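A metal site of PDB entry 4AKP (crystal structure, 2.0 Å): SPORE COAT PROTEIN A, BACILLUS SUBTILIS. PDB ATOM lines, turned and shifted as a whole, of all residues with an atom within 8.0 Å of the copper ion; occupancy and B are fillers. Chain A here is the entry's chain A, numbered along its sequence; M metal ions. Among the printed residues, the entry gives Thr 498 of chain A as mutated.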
ATOM      1  N   PRO A 226     -25.355 -13.924  15.247  1.00  0.00           N
ATOM      2  CA  PRO A 226     -25.482 -13.040  16.425  1.00  0.00           C
ATOM      3  C   PRO A 226     -26.632 -13.375  17.387  1.00  0.00           C
ATOM      4  O   PRO A 226     -26.737 -12.780  18.461  1.00  0.00           O
ATOM      5  CB  PRO A 226     -25.692 -11.650  15.806  1.00  0.00           C
ATOM      6  CG  PRO A 226     -26.304 -11.925  14.458  1.00  0.00           C
ATOM      7  CD  PRO A 226     -25.933 -13.325  14.035  1.00  0.00           C
ATOM      8  N   LEU A 374     -22.615  -1.055  26.715  1.00  0.00           N
ATOM      9  CA  LEU A 374     -22.810  -2.210  25.874  1.00  0.00           C
ATOM     10  C   LEU A 374     -22.647  -1.740  24.435  1.00  0.00           C
ATOM     11  O   LEU A 374     -23.486  -1.016  23.912  1.00  0.00           O
ATOM     12  CB  LEU A 374     -24.189  -2.849  26.114  1.00  0.00           C
ATOM     13  CG  LEU A 374     -24.553  -3.143  27.586  1.00  0.00           C
ATOM     14  CD1 LEU A 374     -25.925  -3.831  27.731  1.00  0.00           C
ATOM     15  CD2 LEU A 374     -23.448  -3.953  28.291  1.00  0.00           C
ATOM     16  N   LEU A 386     -19.758  -8.017  19.504  1.00  0.00           N
ATOM     17  CA  LEU A 386     -20.391  -7.351  20.636  1.00  0.00           C
ATOM     18  C   LEU A 386     -19.390  -7.230  21.780  1.00  0.00           C
ATOM     19  O   LEU A 386     -18.729  -8.217  22.123  1.00  0.00           O
ATOM     20  CB  LEU A 386     -21.675  -8.066  21.063  1.00  0.00           C
ATOM     21  CG  LEU A 386     -22.790  -8.024  20.014  1.00  0.00           C
ATOM     22  CD1 LEU A 386     -22.627  -9.099  18.936  1.00  0.00           C
ATOM     23  CD2 LEU A 386     -24.147  -8.153  20.659  1.00  0.00           C
ATOM     24  N   LEU A 387     -19.264  -6.025  22.331  1.00  0.00           N
ATOM     25  CA  LEU A 387     -18.205  -5.706  23.279  1.00  0.00           C
ATOM     26  C   LEU A 387     -18.716  -4.985  24.523  1.00  0.00           C
ATOM     27  O   LEU A 387     -19.574  -4.110  24.431  1.00  0.00           O
ATOM     28  CB  LEU A 387     -17.108  -4.852  22.599  1.00  0.00           C
ATOM     29  CG  LEU A 387     -16.346  -5.421  21.394  1.00  0.00           C
ATOM     30  CD1 LEU A 387     -15.286  -4.430  20.900  1.00  0.00           C
ATOM     31  CD2 LEU A 387     -15.713  -6.770  21.713  1.00  0.00           C
ATOM     32  N   LEU A 388     -18.187  -5.388  25.676  1.00  0.00           N
ATOM     33  CA  LEU A 388     -18.399  -4.648  26.914  1.00  0.00           C
ATOM     34  C   LEU A 388     -17.309  -3.566  26.957  1.00  0.00           C
ATOM     35  O   LEU A 388     -16.123  -3.895  26.865  1.00  0.00           O
ATOM     36  CB  LEU A 388     -18.303  -5.580  28.128  1.00  0.00           C
ATOM     37  CG  LEU A 388     -19.237  -6.809  28.135  1.00  0.00           C
ATOM     38  CD1 LEU A 388     -18.809  -7.825  29.211  1.00  0.00           C
ATOM     39  CD2 LEU A 388     -20.683  -6.397  28.326  1.00  0.00           C
ATOM     40  N   ASN A 413     -26.988   0.952  27.922  1.00  0.00           N
ATOM     41  CA  ASN A 413     -27.358   0.169  26.736  1.00  0.00           C
ATOM     42  C   ASN A 413     -27.885   1.035  25.598  1.00  0.00           C
ATOM     43  O   ASN A 413     -29.081   1.322  25.522  1.00  0.00           O
ATOM     44  CB  ASN A 413     -28.375  -0.945  27.096  1.00  0.00           C
ATOM     45  CG  ASN A 413     -28.677  -1.875  25.915  1.00  0.00           C
ATOM     46  OD1 ASN A 413     -28.111  -1.745  24.835  1.00  0.00           O
ATOM     47  ND2 ASN A 413     -29.576  -2.825  26.138  1.00  0.00           N
ATOM     48  N   THR A 415     -27.745  -0.013  22.455  1.00  0.00           N
ATOM     49  CA  THR A 415     -28.040  -0.931  21.336  1.00  0.00           C
ATOM     50  C   THR A 415     -29.548  -1.076  21.167  1.00  0.00           C
ATOM     51  O   THR A 415     -30.317  -0.584  21.990  1.00  0.00           O
ATOM     52  CB  THR A 415     -27.389  -2.326  21.540  1.00  0.00           C
ATOM     53  OG1 THR A 415     -28.081  -3.035  22.586  1.00  0.00           O
ATOM     54  CG2 THR A 415     -25.909  -2.203  21.888  1.00  0.00           C
ATOM     55  N   GLY A 417     -31.305  -3.862  21.368  1.00  0.00           N
ATOM     56  CA  GLY A 417     -31.844  -5.026  22.075  1.00  0.00           C
ATOM     57  C   GLY A 417     -31.499  -5.096  23.552  1.00  0.00           C
ATOM     58  O   GLY A 417     -30.631  -4.362  24.038  1.00  0.00           O
ATOM     59  N   THR A 418     -32.216  -5.961  24.277  1.00  0.00           N
ATOM     60  CA  THR A 418     -31.936  -6.247  25.675  1.00  0.00           C
ATOM     61  C   THR A 418     -30.762  -7.224  25.769  1.00  0.00           C
ATOM     62  O   THR A 418     -30.630  -8.127  24.931  1.00  0.00           O
ATOM     63  CB  THR A 418     -33.157  -6.879  26.376  1.00  0.00           C
ATOM     64  OG1 THR A 418     -34.243  -5.948  26.372  1.00  0.00           O
ATOM     65  CG2 THR A 418     -32.825  -7.228  27.820  1.00  0.00           C
ATOM     66  N   HIS A 419     -29.919  -7.016  26.775  1.00  0.00           N
ATOM     67  CA  HIS A 419     -28.838  -7.952  27.081  1.00  0.00           C
ATOM     68  C   HIS A 419     -28.983  -8.381  28.526  1.00  0.00           C
ATOM     69  O   HIS A 419     -29.003  -7.538  29.422  1.00  0.00           O
ATOM     70  CB  HIS A 419     -27.470  -7.295  26.853  1.00  0.00           C
ATOM     71  CG  HIS A 419     -27.236  -6.873  25.431  1.00  0.00           C
ATOM     72  ND1 HIS A 419     -26.790  -7.742  24.469  1.00  0.00           N
ATOM     73  CD2 HIS A 419     -27.405  -5.673  24.821  1.00  0.00           C
ATOM     74  CE1 HIS A 419     -26.681  -7.098  23.320  1.00  0.00           C
ATOM     75  NE2 HIS A 419     -27.052  -5.841  23.505  1.00  0.00           N
ATOM     76  N   PRO A 420     -29.090  -9.697  28.769  1.00  0.00           N
ATOM     77  CA  PRO A 420     -29.107 -10.179  30.132  1.00  0.00           C
ATOM     78  C   PRO A 420     -27.678 -10.225  30.689  1.00  0.00           C
ATOM     79  O   PRO A 420     -26.909 -11.117  30.353  1.00  0.00           O
ATOM     80  CB  PRO A 420     -29.724 -11.576  30.011  1.00  0.00           C
ATOM     81  CG  PRO A 420     -29.372 -12.030  28.641  1.00  0.00           C
ATOM     82  CD  PRO A 420     -29.241 -10.793  27.786  1.00  0.00           C
ATOM     83  N   ILE A 421     -27.342  -9.252  31.524  1.00  0.00           N
ATOM     84  CA  ILE A 421     -25.980  -9.126  32.038  1.00  0.00           C
ATOM     85  C   ILE A 421     -25.822  -9.958  33.296  1.00  0.00           C
ATOM     86  O   ILE A 421     -26.641  -9.882  34.199  1.00  0.00           O
ATOM     87  CB  ILE A 421     -25.585  -7.639  32.301  1.00  0.00           C
ATOM     88  CG1 ILE A 421     -25.783  -6.797  31.023  1.00  0.00           C
ATOM     89  CG2 ILE A 421     -24.155  -7.525  32.868  1.00  0.00           C
ATOM     90  CD1 ILE A 421     -24.994  -7.302  29.806  1.00  0.00           C
ATOM     91  N   ALA A 469     -30.856  -5.757  30.807  1.00  0.00           N
ATOM     92  CA  ALA A 469     -30.520  -4.373  30.532  1.00  0.00           C
ATOM     93  C   ALA A 469     -31.191  -4.001  29.228  1.00  0.00           C
ATOM     94  O   ALA A 469     -30.697  -4.370  28.156  1.00  0.00           O
ATOM     95  CB  ALA A 469     -29.001  -4.195  30.424  1.00  0.00           C
ATOM     96  N   HIS A 491     -20.470 -11.003  31.880  1.00  0.00           N
ATOM     97  CA  HIS A 491     -20.808 -11.111  30.462  1.00  0.00           C
ATOM     98  C   HIS A 491     -22.295 -10.990  30.184  1.00  0.00           C
ATOM     99  O   HIS A 491     -23.125 -11.086  31.086  1.00  0.00           O
ATOM    100  CB  HIS A 491     -20.293 -12.432  29.863  1.00  0.00           C
ATOM    101  CG  HIS A 491     -20.767 -13.672  30.563  1.00  0.00           C
ATOM    102  ND1 HIS A 491     -21.847 -14.415  30.128  1.00  0.00           N
ATOM    103  CD2 HIS A 491     -20.281 -14.314  31.656  1.00  0.00           C
ATOM    104  CE1 HIS A 491     -22.016 -15.457  30.925  1.00  0.00           C
ATOM    105  NE2 HIS A 491     -21.080 -15.425  31.854  1.00  0.00           N
ATOM    106  N   CYS A 492     -22.628 -10.773  28.916  1.00  0.00           N
ATOM    107  CA  CYS A 492     -24.008 -10.989  28.471  1.00  0.00           C
ATOM    108  C   CYS A 492     -24.238 -12.494  28.363  1.00  0.00           C
ATOM    109  O   CYS A 492     -23.352 -13.232  27.899  1.00  0.00           O
ATOM    110  CB  CYS A 492     -24.232 -10.331  27.119  1.00  0.00           C
ATOM    111  SG  CYS A 492     -25.798 -10.771  26.418  1.00  0.00           S
ATOM    112  N   HIS A 493     -25.417 -12.952  28.805  1.00  0.00           N
ATOM    113  CA  HIS A 493     -25.727 -14.385  28.824  1.00  0.00           C
ATOM    114  C   HIS A 493     -26.534 -14.858  27.595  1.00  0.00           C
ATOM    115  O   HIS A 493     -27.093 -15.952  27.594  1.00  0.00           O
ATOM    116  CB  HIS A 493     -26.397 -14.822  30.135  1.00  0.00           C
ATOM    117  CG  HIS A 493     -25.933 -16.163  30.640  1.00  0.00           C
ATOM    118  ND1 HIS A 493     -26.195 -17.341  29.965  1.00  0.00           N
ATOM    119  CD2 HIS A 493     -25.235 -16.511  31.756  1.00  0.00           C
ATOM    120  CE1 HIS A 493     -25.668 -18.355  30.642  1.00  0.00           C
ATOM    121  NE2 HIS A 493     -25.085 -17.880  31.731  1.00  0.00           N
ATOM    122  N   ILE A 494     -26.592 -14.024  26.553  1.00  0.00           N
ATOM    123  CA  ILE A 494     -26.953 -14.486  25.214  1.00  0.00           C
ATOM    124  C   ILE A 494     -25.678 -15.099  24.659  1.00  0.00           C
ATOM    125  O   ILE A 494     -24.703 -14.381  24.391  1.00  0.00           O
ATOM    126  CB  ILE A 494     -27.504 -13.365  24.296  1.00  0.00           C
ATOM    127  CG1 ILE A 494     -28.886 -12.912  24.777  1.00  0.00           C
ATOM    128  CG2 ILE A 494     -27.577 -13.833  22.816  1.00  0.00           C
ATOM    129  CD1 ILE A 494     -29.364 -11.601  24.177  1.00  0.00           C
ATOM    130  N   LEU A 495     -25.666 -16.412  24.514  1.00  0.00           N
ATOM    131  CA  LEU A 495     -24.420 -17.155  24.285  1.00  0.00           C
ATOM    132  C   LEU A 495     -23.754 -16.818  22.952  1.00  0.00           C
ATOM    133  O   LEU A 495     -22.523 -16.850  22.847  1.00  0.00           O
ATOM    134  CB  LEU A 495     -24.653 -18.662  24.449  1.00  0.00           C
ATOM    135  CG  LEU A 495     -25.207 -19.067  25.820  1.00  0.00           C
ATOM    136  CD1 LEU A 495     -25.326 -20.569  25.919  1.00  0.00           C
ATOM    137  CD2 LEU A 495     -24.361 -18.514  26.978  1.00  0.00           C
ATOM    138  N   GLU A 496     -24.557 -16.489  21.950  1.00  0.00           N
ATOM    139  CA  GLU A 496     -24.052 -16.006  20.667  1.00  0.00           C
ATOM    140  C   GLU A 496     -23.323 -14.666  20.816  1.00  0.00           C
ATOM    141  O   GLU A 496     -22.450 -14.336  20.004  1.00  0.00           O
ATOM    142  CB  GLU A 496     -25.214 -15.882  19.667  1.00  0.00           C
ATOM    143  CG  GLU A 496     -25.670 -17.232  19.064  1.00  0.00           C
ATOM    144  CD  GLU A 496     -26.418 -18.130  20.056  1.00  0.00           C
ATOM    145  OE1 GLU A 496     -26.996 -17.604  21.032  1.00  0.00           O
ATOM    146  OE2 GLU A 496     -26.429 -19.369  19.858  1.00  0.00           O
ATOM    147  N   HIS A 497     -23.667 -13.900  21.850  1.00  0.00           N
ATOM    148  CA  HIS A 497     -22.972 -12.645  22.189  1.00  0.00           C
ATOM    149  C   HIS A 497     -21.764 -12.934  23.061  1.00  0.00           C
ATOM    150  O   HIS A 497     -20.694 -12.348  22.852  1.00  0.00           O
ATOM    151  CB  HIS A 497     -23.895 -11.692  22.950  1.00  0.00           C
ATOM    152  CG  HIS A 497     -25.067 -11.217  22.142  1.00  0.00           C
ATOM    153  ND1 HIS A 497     -25.975 -10.293  22.637  1.00  0.00           N
ATOM    154  CD2 HIS A 497     -25.481 -11.512  20.890  1.00  0.00           C
ATOM    155  CE1 HIS A 497     -26.898 -10.064  21.730  1.00  0.00           C
ATOM    156  NE2 HIS A 497     -26.625 -10.778  20.648  1.00  0.00           N
ATOM    157  N   THR A 498     -21.931 -13.814  24.038  1.00  0.00           N
ATOM    158  CA  THR A 498     -20.858 -14.226  24.950  1.00  0.00           C
ATOM    159  C   THR A 498     -19.595 -14.645  24.197  1.00  0.00           C
ATOM    160  O   THR A 498     -18.471 -14.254  24.561  1.00  0.00           O
ATOM    161  CB  THR A 498     -21.306 -15.399  25.861  1.00  0.00           C
ATOM    162  OG1 THR A 498     -22.610 -15.129  26.394  1.00  0.00           O
ATOM    163  CG2 THR A 498     -20.328 -15.582  27.008  1.00  0.00           C
ATOM    164  N   MET A 502     -18.680 -10.639  23.984  1.00  0.00           N
ATOM    165  CA  MET A 502     -19.317  -9.821  25.023  1.00  0.00           C
ATOM    166  C   MET A 502     -19.102 -10.384  26.426  1.00  0.00           C
ATOM    167  O   MET A 502     -20.048 -10.612  27.187  1.00  0.00           O
ATOM    168  CB  MET A 502     -20.807  -9.658  24.729  1.00  0.00           C
ATOM    169  CG  MET A 502     -21.396  -8.386  25.269  1.00  0.00           C
ATOM    170  SD  MET A 502     -23.026  -8.075  24.584  1.00  0.00           S
ATOM    171  CE  MET A 502     -23.463  -6.615  25.495  1.00  0.00           C
HETATM  172 CU    CU M   1     -25.945  -9.558  24.490  1.00  0.00          CU
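Ile 494 touches the copper ion. Met 502 touches the copper ion (SD to CU, 3.3 Å). Five residues have an atom within 4 Å of the copper ion: His 419, Cys 492, Ile 494, His 497 and Met 502. The nearest printed residue that does not touch the copper ion is Leu 386 (4.5 Å).
The copper ion is bound by ND1 of His 497 (2.0 Å), ND1 of His 419 (2.0 Å) and SG of Cys 492 (2.3 Å).
The backbone carbonyl oxygen (O) of Cys 492 is in hydrogen-bond range of the side-chain hydroxyl (OG1) of Thr 498, 2.5 Å away. The backbone NH (N) of Ala 469 sits at hydrogen-bond distance from the backbone carbonyl oxygen (O) of His 419, at 2.9 Å. N of Met 502 sits at hydrogen-bond distance from O of His 497. The backbone NH of Cys 492 lies within hydrogen-bond range of the backbone carbonyl oxygen of Met 502, 3.1 Å away. SG of Cys 492 sits close to N of Ile 494, 3.4 Å away. SD of Met 502 sits close to ND1 of His 419, at 3.8 Å. NE2 of His 497 is in hydrogen-bond range of O of Pro 226 (3.0 Å). The backbone carbonyl oxygen (O) of Leu 386 sits at hydrogen-bond distance from the backbone NH (N) of Met 502 (3.1 Å).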
